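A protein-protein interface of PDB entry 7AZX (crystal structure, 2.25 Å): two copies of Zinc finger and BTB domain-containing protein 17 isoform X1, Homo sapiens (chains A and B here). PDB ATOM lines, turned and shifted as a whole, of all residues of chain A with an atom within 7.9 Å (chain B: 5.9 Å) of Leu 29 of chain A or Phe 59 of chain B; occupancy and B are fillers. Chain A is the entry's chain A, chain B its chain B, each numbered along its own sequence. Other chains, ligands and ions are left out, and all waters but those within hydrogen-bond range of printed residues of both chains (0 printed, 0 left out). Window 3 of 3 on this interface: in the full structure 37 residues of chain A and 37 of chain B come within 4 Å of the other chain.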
ATOM      1  N   LEU A  20     -26.170  -2.087 -14.880  1.00  0.00           N
ATOM      2  CA  LEU A  20     -27.165  -1.113 -14.444  1.00  0.00           C
ATOM      3  C   LEU A  20     -28.207  -1.750 -13.534  1.00  0.00           C
ATOM      4  O   LEU A  20     -28.724  -1.090 -12.626  1.00  0.00           O
ATOM      5  CB  LEU A  20     -27.845  -0.475 -15.656  1.00  0.00           C
ATOM      6  CG  LEU A  20     -26.983   0.439 -16.529  1.00  0.00           C
ATOM      7  CD1 LEU A  20     -27.800   0.990 -17.688  1.00  0.00           C
ATOM      8  CD2 LEU A  20     -26.388   1.568 -15.702  1.00  0.00           C
ATOM      9  N   GLN A  23     -26.567  -2.237 -10.004  1.00  0.00           N
ATOM     10  CA  GLN A  23     -26.532  -0.954  -9.307  1.00  0.00           C
ATOM     11  C   GLN A  23     -27.895  -0.617  -8.716  1.00  0.00           C
ATOM     12  O   GLN A  23     -27.985  -0.110  -7.592  1.00  0.00           O
ATOM     13  CB  GLN A  23     -26.077   0.155 -10.259  1.00  0.00           C
ATOM     14  CG  GLN A  23     -24.667  -0.008 -10.800  1.00  0.00           C
ATOM     15  CD  GLN A  23     -24.343   1.004 -11.884  1.00  0.00           C
ATOM     16  OE1 GLN A  23     -24.993   2.044 -11.992  1.00  0.00           O
ATOM     17  NE2 GLN A  23     -23.338   0.700 -12.699  1.00  0.00           N
ATOM     18  N   ARG A  24     -28.967  -0.897  -9.460  1.00  0.00           N
ATOM     19  CA  ARG A  24     -30.309  -0.591  -8.978  1.00  0.00           C
ATOM     20  C   ARG A  24     -30.694  -1.482  -7.802  1.00  0.00           C
ATOM     21  O   ARG A  24     -31.299  -1.010  -6.833  1.00  0.00           O
ATOM     22  CB  ARG A  24     -31.314  -0.733 -10.121  1.00  0.00           C
ATOM     23  CG  ARG A  24     -32.685  -1.235  -9.704  1.00  0.00           C
ATOM     24  CD  ARG A  24     -33.216  -2.260 -10.692  1.00  0.00           C
ATOM     25  NE  ARG A  24     -34.475  -2.850 -10.245  1.00  0.00           N
ATOM     26  CZ  ARG A  24     -35.027  -3.930 -10.785  1.00  0.00           C
ATOM     27  NH1 ARG A  24     -34.432  -4.547 -11.797  1.00  0.00           N
ATOM     28  NH2 ARG A  24     -36.176  -4.396 -10.314  1.00  0.00           N
ATOM     29  N   LEU A  26     -28.780  -2.689  -5.608  1.00  0.00           N
ATOM     30  CA  LEU A  26     -28.020  -2.237  -4.453  1.00  0.00           C
ATOM     31  C   LEU A  26     -28.153  -0.740  -4.210  1.00  0.00           C
ATOM     32  O   LEU A  26     -27.516  -0.217  -3.291  1.00  0.00           O
ATOM     33  CB  LEU A  26     -26.541  -2.604  -4.615  1.00  0.00           C
ATOM     34  CG  LEU A  26     -26.192  -4.084  -4.448  1.00  0.00           C
ATOM     35  CD1 LEU A  26     -24.749  -4.345  -4.854  1.00  0.00           C
ATOM     36  CD2 LEU A  26     -26.444  -4.536  -3.019  1.00  0.00           C
ATOM     37  N   GLY A  27     -28.959  -0.042  -5.008  1.00  0.00           N
ATOM     38  CA  GLY A  27     -29.135   1.385  -4.832  1.00  0.00           C
ATOM     39  C   GLY A  27     -27.915   2.220  -5.146  1.00  0.00           C
ATOM     40  O   GLY A  27     -27.816   3.354  -4.671  1.00  0.00           O
ATOM     41  N   LEU A  28     -26.982   1.693  -5.934  1.00  0.00           N
ATOM     42  CA  LEU A  28     -25.758   2.413  -6.250  1.00  0.00           C
ATOM     43  C   LEU A  28     -25.993   3.367  -7.414  1.00  0.00           C
ATOM     44  O   LEU A  28     -26.555   2.977  -8.444  1.00  0.00           O
ATOM     45  CB  LEU A  28     -24.637   1.432  -6.588  1.00  0.00           C
ATOM     46  CG  LEU A  28     -24.282   0.419  -5.497  1.00  0.00           C
ATOM     47  CD1 LEU A  28     -23.239  -0.570  -5.998  1.00  0.00           C
ATOM     48  CD2 LEU A  28     -23.796   1.129  -4.244  1.00  0.00           C
ATOM     49  N   LEU A  29     -25.561   4.619  -7.245  1.00  0.00           N
ATOM     50  CA  LEU A  29     -25.662   5.650  -8.279  1.00  0.00           C
ATOM     51  C   LEU A  29     -27.104   5.868  -8.732  1.00  0.00           C
ATOM     52  O   LEU A  29     -27.358   6.190  -9.895  1.00  0.00           O
ATOM     53  CB  LEU A  29     -24.772   5.319  -9.482  1.00  0.00           C
ATOM     54  CG  LEU A  29     -23.292   5.080  -9.179  1.00  0.00           C
ATOM     55  CD1 LEU A  29     -22.541   4.681 -10.440  1.00  0.00           C
ATOM     56  CD2 LEU A  29     -22.670   6.316  -8.547  1.00  0.00           C
ATOM     57  N   CYS A  30     -28.056   5.697  -7.821  1.00  0.00           N
ATOM     58  CA  CYS A  30     -29.470   5.873  -8.123  1.00  0.00           C
ATOM     59  C   CYS A  30     -29.909   7.261  -7.674  1.00  0.00           C
ATOM     60  O   CYS A  30     -29.823   7.592  -6.486  1.00  0.00           O
ATOM     61  CB  CYS A  30     -30.310   4.792  -7.445  1.00  0.00           C
ATOM     62  SG  CYS A  30     -30.074   3.141  -8.141  1.00  0.00           S
ATOM     63  N   ASP A  31     -30.372   8.068  -8.626  1.00  0.00           N
ATOM     64  CA  ASP A  31     -30.878   9.404  -8.347  1.00  0.00           C
ATOM     65  C   ASP A  31     -32.400   9.454  -8.319  1.00  0.00           C
ATOM     66  O   ASP A  31     -32.974  10.547  -8.300  1.00  0.00           O
ATOM     67  CB  ASP A  31     -30.340  10.400  -9.376  1.00  0.00           C
ATOM     68  CG  ASP A  31     -30.609   9.966 -10.803  1.00  0.00           C
ATOM     69  OD1 ASP A  31     -31.092   8.832 -11.003  1.00  0.00           O
ATOM     70  OD2 ASP A  31     -30.337  10.760 -11.728  1.00  0.00           O
ATOM     71  N   CYS A  32     -33.061   8.299  -8.319  1.00  0.00           N
ATOM     72  CA  CYS A  32     -34.517   8.227  -8.329  1.00  0.00           C
ATOM     73  C   CYS A  32     -34.967   7.121  -7.389  1.00  0.00           C
ATOM     74  O   CYS A  32     -34.456   6.000  -7.459  1.00  0.00           O
ATOM     75  CB  CYS A  32     -35.048   7.968  -9.744  1.00  0.00           C
ATOM     76  SG  CYS A  32     -36.739   8.538 -10.022  1.00  0.00           S
ATOM     77  N   LYS A  42     -35.548   1.920  -6.195  1.00  0.00           N
ATOM     78  CA  LYS A  42     -34.500   2.826  -6.641  1.00  0.00           C
ATOM     79  C   LYS A  42     -34.139   2.523  -8.089  1.00  0.00           C
ATOM     80  O   LYS A  42     -34.114   1.360  -8.500  1.00  0.00           O
ATOM     81  CB  LYS A  42     -33.262   2.712  -5.750  1.00  0.00           C
ATOM     82  CG  LYS A  42     -33.558   2.831  -4.263  1.00  0.00           C
ATOM     83  CD  LYS A  42     -32.291   3.080  -3.458  1.00  0.00           C
ATOM     84  CE  LYS A  42     -31.748   4.481  -3.695  1.00  0.00           C
ATOM     85  NZ  LYS A  42     -30.566   4.773  -2.835  1.00  0.00           N
ATOM     86  N   ALA A  43     -33.865   3.573  -8.859  1.00  0.00           N
ATOM     87  CA  ALA A  43     -33.563   3.418 -10.276  1.00  0.00           C
ATOM     88  C   ALA A  43     -32.794   4.640 -10.755  1.00  0.00           C
ATOM     89  O   ALA A  43     -32.628   5.622 -10.027  1.00  0.00           O
ATOM     90  CB  ALA A  43     -34.840   3.217 -11.098  1.00  0.00           C
ATOM     91  N   HIS A  44     -32.321   4.564 -11.997  1.00  0.00           N
ATOM     92  CA  HIS A  44     -31.615   5.663 -12.642  1.00  0.00           C
ATOM     93  C   HIS A  44     -32.585   6.435 -13.524  1.00  0.00           C
ATOM     94  O   HIS A  44     -33.350   5.835 -14.286  1.00  0.00           O
ATOM     95  CB  HIS A  44     -30.443   5.154 -13.484  1.00  0.00           C
ATOM     96  CG  HIS A  44     -29.594   4.131 -12.797  1.00  0.00           C
ATOM     97  ND1 HIS A  44     -29.881   2.783 -12.828  1.00  0.00           N
ATOM     98  CD2 HIS A  44     -28.454   4.256 -12.076  1.00  0.00           C
ATOM     99  CE1 HIS A  44     -28.960   2.123 -12.148  1.00  0.00           C
ATOM    100  NE2 HIS A  44     -28.083   2.993 -11.682  1.00  0.00           N
ATOM    101  N   LYS A  45     -32.545   7.767 -13.427  1.00  0.00           N
ATOM    102  CA  LYS A  45     -33.424   8.591 -14.249  1.00  0.00           C
ATOM    103  C   LYS A  45     -33.088   8.469 -15.730  1.00  0.00           C
ATOM    104  O   LYS A  45     -33.965   8.661 -16.580  1.00  0.00           O
ATOM    105  CB  LYS A  45     -33.345  10.052 -13.802  1.00  0.00           C
ATOM    106  CG  LYS A  45     -33.859  10.287 -12.389  1.00  0.00           C
ATOM    107  CD  LYS A  45     -34.274  11.733 -12.169  1.00  0.00           C
ATOM    108  CE  LYS A  45     -33.069  12.635 -11.957  1.00  0.00           C
ATOM    109  NZ  LYS A  45     -33.471  13.984 -11.465  1.00  0.00           N
ATOM    110  N   ALA A  46     -31.834   8.147 -16.058  1.00  0.00           N
ATOM    111  CA  ALA A  46     -31.464   7.962 -17.457  1.00  0.00           C
ATOM    112  C   ALA A  46     -32.049   6.678 -18.027  1.00  0.00           C
ATOM    113  O   ALA A  46     -32.399   6.631 -19.213  1.00  0.00           O
ATOM    114  CB  ALA A  46     -29.942   7.963 -17.603  1.00  0.00           C
ATOM    115  N   TYR A  84     -34.570  -3.240 -16.573  1.00  0.00           N
ATOM    116  CA  TYR A  84     -33.189  -3.586 -16.269  1.00  0.00           C
ATOM    117  C   TYR A  84     -32.818  -5.013 -16.650  1.00  0.00           C
ATOM    118  O   TYR A  84     -31.641  -5.376 -16.543  1.00  0.00           O
ATOM    119  CB  TYR A  84     -32.912  -3.370 -14.776  1.00  0.00           C
ATOM    120  CG  TYR A  84     -32.819  -1.913 -14.378  1.00  0.00           C
ATOM    121  CD1 TYR A  84     -33.953  -1.196 -14.020  1.00  0.00           C
ATOM    122  CD2 TYR A  84     -31.595  -1.254 -14.361  1.00  0.00           C
ATOM    123  CE1 TYR A  84     -33.872   0.137 -13.656  1.00  0.00           C
ATOM    124  CE2 TYR A  84     -31.504   0.076 -13.998  1.00  0.00           C
ATOM    125  CZ  TYR A  84     -32.644   0.768 -13.647  1.00  0.00           C
ATOM    126  OH  TYR A  84     -32.556   2.093 -13.284  1.00  0.00           O
ATOM    127  N   CYS B  32     -21.952  13.874 -15.772  1.00  0.00           N
ATOM    128  CA  CYS B  32     -20.517  13.912 -15.999  1.00  0.00           C
ATOM    129  C   CYS B  32     -20.213  14.822 -17.181  1.00  0.00           C
ATOM    130  O   CYS B  32     -21.013  14.941 -18.115  1.00  0.00           O
ATOM    131  CB  CYS B  32     -19.956  12.510 -16.270  1.00  0.00           C
ATOM    132  SG  CYS B  32     -19.811  11.463 -14.807  1.00  0.00           S
ATOM    133  N   HIS B  44     -22.873   9.656 -18.465  1.00  0.00           N
ATOM    134  CA  HIS B  44     -23.560   9.288 -17.235  1.00  0.00           C
ATOM    135  C   HIS B  44     -22.606   8.520 -16.330  1.00  0.00           C
ATOM    136  O   HIS B  44     -21.879   7.636 -16.790  1.00  0.00           O
ATOM    137  CB  HIS B  44     -24.796   8.431 -17.522  1.00  0.00           C
ATOM    138  CG  HIS B  44     -25.661   8.957 -18.625  1.00  0.00           C
ATOM    139  ND1 HIS B  44     -25.355   8.786 -19.958  1.00  0.00           N
ATOM    140  CD2 HIS B  44     -26.831   9.638 -18.592  1.00  0.00           C
ATOM    141  CE1 HIS B  44     -26.295   9.347 -20.698  1.00  0.00           C
ATOM    142  NE2 HIS B  44     -27.202   9.871 -19.894  1.00  0.00           N
ATOM    143  N   LYS B  45     -22.617   8.858 -15.038  1.00  0.00           N
ATOM    144  CA  LYS B  45     -21.731   8.174 -14.102  1.00  0.00           C
ATOM    145  C   LYS B  45     -22.126   6.714 -13.916  1.00  0.00           C
ATOM    146  O   LYS B  45     -21.277   5.883 -13.573  1.00  0.00           O
ATOM    147  CB  LYS B  45     -21.716   8.901 -12.757  1.00  0.00           C
ATOM    148  CG  LYS B  45     -23.055   8.932 -12.041  1.00  0.00           C
ATOM    149  CD  LYS B  45     -22.955   9.660 -10.707  1.00  0.00           C
ATOM    150  CE  LYS B  45     -22.448  11.083 -10.888  1.00  0.00           C
ATOM    151  NZ  LYS B  45     -22.498  11.858  -9.617  1.00  0.00           N
ATOM    152  N   ALA B  46     -23.400   6.380 -14.140  1.00  0.00           N
ATOM    153  CA  ALA B  46     -23.824   4.988 -14.033  1.00  0.00           C
ATOM    154  C   ALA B  46     -23.347   4.165 -15.222  1.00  0.00           C
ATOM    155  O   ALA B  46     -23.081   2.965 -15.078  1.00  0.00           O
ATOM    156  CB  ALA B  46     -25.345   4.907 -13.906  1.00  0.00           C
ATOM    157  N   LEU B  48     -20.511   4.889 -16.968  1.00  0.00           N
ATOM    158  CA  LEU B  48     -19.063   4.777 -16.828  1.00  0.00           C
ATOM    159  C   LEU B  48     -18.688   3.676 -15.845  1.00  0.00           C
ATOM    160  O   LEU B  48     -17.782   2.877 -16.112  1.00  0.00           O
ATOM    161  CB  LEU B  48     -18.474   6.116 -16.382  1.00  0.00           C
ATOM    162  CG  LEU B  48     -18.740   7.322 -17.283  1.00  0.00           C
ATOM    163  CD1 LEU B  48     -18.156   8.586 -16.672  1.00  0.00           C
ATOM    164  CD2 LEU B  48     -18.185   7.091 -18.680  1.00  0.00           C
ATOM    165  N   ALA B  49     -19.374   3.618 -14.702  1.00  0.00           N
ATOM    166  CA  ALA B  49     -19.113   2.553 -13.740  1.00  0.00           C
ATOM    167  C   ALA B  49     -19.485   1.189 -14.304  1.00  0.00           C
ATOM    168  O   ALA B  49     -18.870   0.179 -13.943  1.00  0.00           O
ATOM    169  CB  ALA B  49     -19.876   2.821 -12.443  1.00  0.00           C
ATOM    170  N   TYR B  54     -12.289   1.277 -13.278  1.00  0.00           N
ATOM    171  CA  TYR B  54     -11.731   2.490 -12.687  1.00  0.00           C
ATOM    172  C   TYR B  54     -12.837   3.466 -12.303  1.00  0.00           C
ATOM    173  O   TYR B  54     -12.869   3.978 -11.178  1.00  0.00           O
ATOM    174  CB  TYR B  54     -10.747   3.144 -13.659  1.00  0.00           C
ATOM    175  CG  TYR B  54     -10.264   4.510 -13.220  1.00  0.00           C
ATOM    176  CD1 TYR B  54      -9.198   4.640 -12.340  1.00  0.00           C
ATOM    177  CD2 TYR B  54     -10.874   5.668 -13.688  1.00  0.00           C
ATOM    178  CE1 TYR B  54      -8.753   5.886 -11.937  1.00  0.00           C
ATOM    179  CE2 TYR B  54     -10.436   6.917 -13.289  1.00  0.00           C
ATOM    180  CZ  TYR B  54      -9.376   7.020 -12.415  1.00  0.00           C
ATOM    181  OH  TYR B  54      -8.936   8.263 -12.016  1.00  0.00           O
ATOM    182  N   PHE B  55     -13.757   3.736 -13.233  1.00  0.00           N
ATOM    183  CA  PHE B  55     -14.866   4.633 -12.932  1.00  0.00           C
ATOM    184  C   PHE B  55     -15.828   4.015 -11.926  1.00  0.00           C
ATOM    185  O   PHE B  55     -16.528   4.743 -11.213  1.00  0.00           O
ATOM    186  CB  PHE B  55     -15.602   5.009 -14.217  1.00  0.00           C
ATOM    187  CG  PHE B  55     -14.949   6.124 -14.978  1.00  0.00           C
ATOM    188  CD1 PHE B  55     -14.456   7.236 -14.315  1.00  0.00           C
ATOM    189  CD2 PHE B  55     -14.818   6.058 -16.355  1.00  0.00           C
ATOM    190  CE1 PHE B  55     -13.851   8.264 -15.011  1.00  0.00           C
ATOM    191  CE2 PHE B  55     -14.212   7.083 -17.056  1.00  0.00           C
ATOM    192  CZ  PHE B  55     -13.727   8.187 -16.383  1.00  0.00           C
ATOM    193  N   LYS B  56     -15.879   2.683 -11.854  1.00  0.00           N
ATOM    194  CA  LYS B  56     -16.688   2.026 -10.834  1.00  0.00           C
ATOM    195  C   LYS B  56     -16.182   2.375  -9.440  1.00  0.00           C
ATOM    196  O   LYS B  56     -16.923   2.919  -8.614  1.00  0.00           O
ATOM    197  CB  LYS B  56     -16.682   0.512 -11.051  1.00  0.00           C
ATOM    198  CG  LYS B  56     -17.792  -0.222 -10.315  1.00  0.00           C
ATOM    199  CD  LYS B  56     -17.509  -1.714 -10.233  1.00  0.00           C
ATOM    200  CE  LYS B  56     -18.706  -2.474  -9.684  1.00  0.00           C
ATOM    201  NZ  LYS B  56     -19.790  -2.611 -10.696  1.00  0.00           N
ATOM    202  N   MET B  57     -14.907   2.079  -9.168  1.00  0.00           N
ATOM    203  CA  MET B  57     -14.318   2.420  -7.876  1.00  0.00           C
ATOM    204  C   MET B  57     -14.396   3.915  -7.598  1.00  0.00           C
ATOM    205  O   MET B  57     -14.523   4.326  -6.439  1.00  0.00           O
ATOM    206  CB  MET B  57     -12.862   1.958  -7.826  1.00  0.00           C
ATOM    207  CG  MET B  57     -12.649   0.496  -8.178  1.00  0.00           C
ATOM    208  SD  MET B  57     -10.900   0.053  -8.219  1.00  0.00           S
ATOM    209  CE  MET B  57     -10.274   1.254  -9.394  1.00  0.00           C
ATOM    210  N   LEU B  58     -14.327   4.740  -8.644  1.00  0.00           N
ATOM    211  CA  LEU B  58     -14.346   6.186  -8.462  1.00  0.00           C
ATOM    212  C   LEU B  58     -15.728   6.713  -8.101  1.00  0.00           C
ATOM    213  O   LEU B  58     -15.829   7.814  -7.548  1.00  0.00           O
ATOM    214  CB  LEU B  58     -13.844   6.875  -9.733  1.00  0.00           C
ATOM    215  CG  LEU B  58     -13.367   8.323  -9.606  1.00  0.00           C
ATOM    216  CD1 LEU B  58     -11.945   8.374  -9.069  1.00  0.00           C
ATOM    217  CD2 LEU B  58     -13.467   9.039 -10.945  1.00  0.00           C
ATOM    218  N   PHE B  59     -16.789   5.961  -8.387  1.00  0.00           N
ATOM    219  CA  PHE B  59     -18.148   6.461  -8.225  1.00  0.00           C
ATOM    220  C   PHE B  59     -18.938   5.789  -7.114  1.00  0.00           C
ATOM    221  O   PHE B  59     -19.780   6.445  -6.497  1.00  0.00           O
ATOM    222  CB  PHE B  59     -18.922   6.324  -9.542  1.00  0.00           C
ATOM    223  CG  PHE B  59     -18.469   7.279 -10.609  1.00  0.00           C
ATOM    224  CD1 PHE B  59     -17.837   8.464 -10.269  1.00  0.00           C
ATOM    225  CD2 PHE B  59     -18.671   6.995 -11.950  1.00  0.00           C
ATOM    226  CE1 PHE B  59     -17.414   9.348 -11.243  1.00  0.00           C
ATOM    227  CE2 PHE B  59     -18.251   7.876 -12.931  1.00  0.00           C
ATOM    228  CZ  PHE B  59     -17.621   9.054 -12.575  1.00  0.00           C
ATOM    229  N   VAL B  60     -18.699   4.506  -6.836  1.00  0.00           N
ATOM    230  CA  VAL B  60     -19.439   3.838  -5.771  1.00  0.00           C
ATOM    231  C   VAL B  60     -18.776   3.994  -4.406  1.00  0.00           C
ATOM    232  O   VAL B  60     -19.442   3.793  -3.380  1.00  0.00           O
ATOM    233  CB  VAL B  60     -19.640   2.340  -6.071  1.00  0.00           C
ATOM    234  CG1 VAL B  60     -20.457   2.151  -7.345  1.00  0.00           C
ATOM    235  CG2 VAL B  60     -18.305   1.619  -6.157  1.00  0.00           C
ATOM    236  N   ASP B  61     -17.491   4.356  -4.360  1.00  0.00           N
ATOM    237  CA  ASP B  61     -16.769   4.470  -3.102  1.00  0.00           C
ATOM    238  C   ASP B  61     -16.162   5.841  -2.841  1.00  0.00           C
ATOM    239  O   ASP B  61     -15.846   6.139  -1.684  1.00  0.00           O
ATOM    240  CB  ASP B  61     -15.637   3.431  -3.030  1.00  0.00           C
ATOM    241  CG  ASP B  61     -16.093   2.038  -3.417  1.00  0.00           C
ATOM    242  OD1 ASP B  61     -16.921   1.455  -2.686  1.00  0.00           O
ATOM    243  OD2 ASP B  61     -15.610   1.522  -4.447  1.00  0.00           O
ATOM    244  N   GLN B  62     -15.987   6.676  -3.863  1.00  0.00           N
ATOM    245  CA  GLN B  62     -15.217   7.903  -3.730  1.00  0.00           C
ATOM    246  C   GLN B  62     -16.002   9.087  -4.282  1.00  0.00           C
ATOM    247  O   GLN B  62     -17.022   8.930  -4.958  1.00  0.00           O
ATOM    248  CB  GLN B  62     -13.864   7.778  -4.445  1.00  0.00           C
ATOM    249  CG  GLN B  62     -12.930   6.766  -3.802  1.00  0.00           C
ATOM    250  CD  GLN B  62     -12.198   5.919  -4.822  1.00  0.00           C
ATOM    251  OE1 GLN B  62     -12.115   6.277  -5.996  1.00  0.00           O
ATOM    252  NE2 GLN B  62     -11.669   4.785  -4.380  1.00  0.00           N
ATOM    253  N   LYS B  63     -15.505  10.284  -3.981  1.00  0.00           N
ATOM    254  CA  LYS B  63     -16.123  11.522  -4.442  1.00  0.00           C
ATOM    255  C   LYS B  63     -15.846  11.756  -5.924  1.00  0.00           C
ATOM    256  O   LYS B  63     -14.706  11.990  -6.323  1.00  0.00           O
ATOM    257  CB  LYS B  63     -15.617  12.710  -3.620  1.00  0.00           C
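Printed residues of chain B that touch a printed residue of chain A: His 44, Lys 45, Ala 46, Ala 49 and Phe 59.
Printed residues of chain A that touch a printed residue of chain B: Leu 20, Gln 23, Leu 29, His 44 and Ala 46.
Along chain A the printed residues that touch a printed residue of chain B span positions 20 to 46.
Among the printed residues, 8 pairs touch across the chains.
Leu 29 of chain A touches just these residues of chain B: Lys 45, Ala 46, Ala 49 and Phe 59.
Of the printed residues of chain B, Ala 46 of chain A touches His 44 (3.7 Å).
Of the printed residues of chain A, Ala 49 of chain B touches Leu 29 (3.8 Å).
Of the printed residues of chain B, Leu 20 of chain A touches Ala 46 (3.6 Å).
Leu 48 of chain B touches none of the printed residues of chain A.
Lys 45 of chain A touches none of the printed residues of chain B.
The nearest printed residue of chain B that does not touch Leu 20 of chain A is Leu 48 of chain B (6.9 Å).
His 44 of chain A touches Ala 46 of chain B, and with the chains exchanged Ala 46 of chain A touches His 44 of chain B.
Of the 8 pairs that touch across the chains among the printed residues, 2 have their exchanged pair printed and touching as well.
The side-chain amide nitrogen (NE2) of Gln 23 of chain A sits at hydrogen-bond distance from the backbone carbonyl oxygen (O) of Ala 46 of chain B (3.3 Å).
The backbone carbonyl oxygen (O) of Gln 23 of chain A is in hydrogen-bond range of the backbone NH (N) of Leu 28 of chain A (2.6 Å).
OE1 of Gln 23 of chain A lies within hydrogen-bond range of NE2 of His 44 of chain A (3.2 Å).
OH of Tyr 84 of chain A sits at hydrogen-bond distance from N of His 44 of chain A, at 2.8 Å.
Among the printed residues, merely in contact across the chains: Leu 29 of chain A with Phe 59 of chain B, Leu 29 of chain A with Lys 45 of chain B, Leu 20 of chain A with Ala 46 of chain B, His 44 of chain A with Ala 46 of chain B, Ala 46 of chain A with His 44 of chain B, Leu 29 of chain A with Ala 49 of chain B and Leu 29 of chain A with Ala 46 of chain B.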
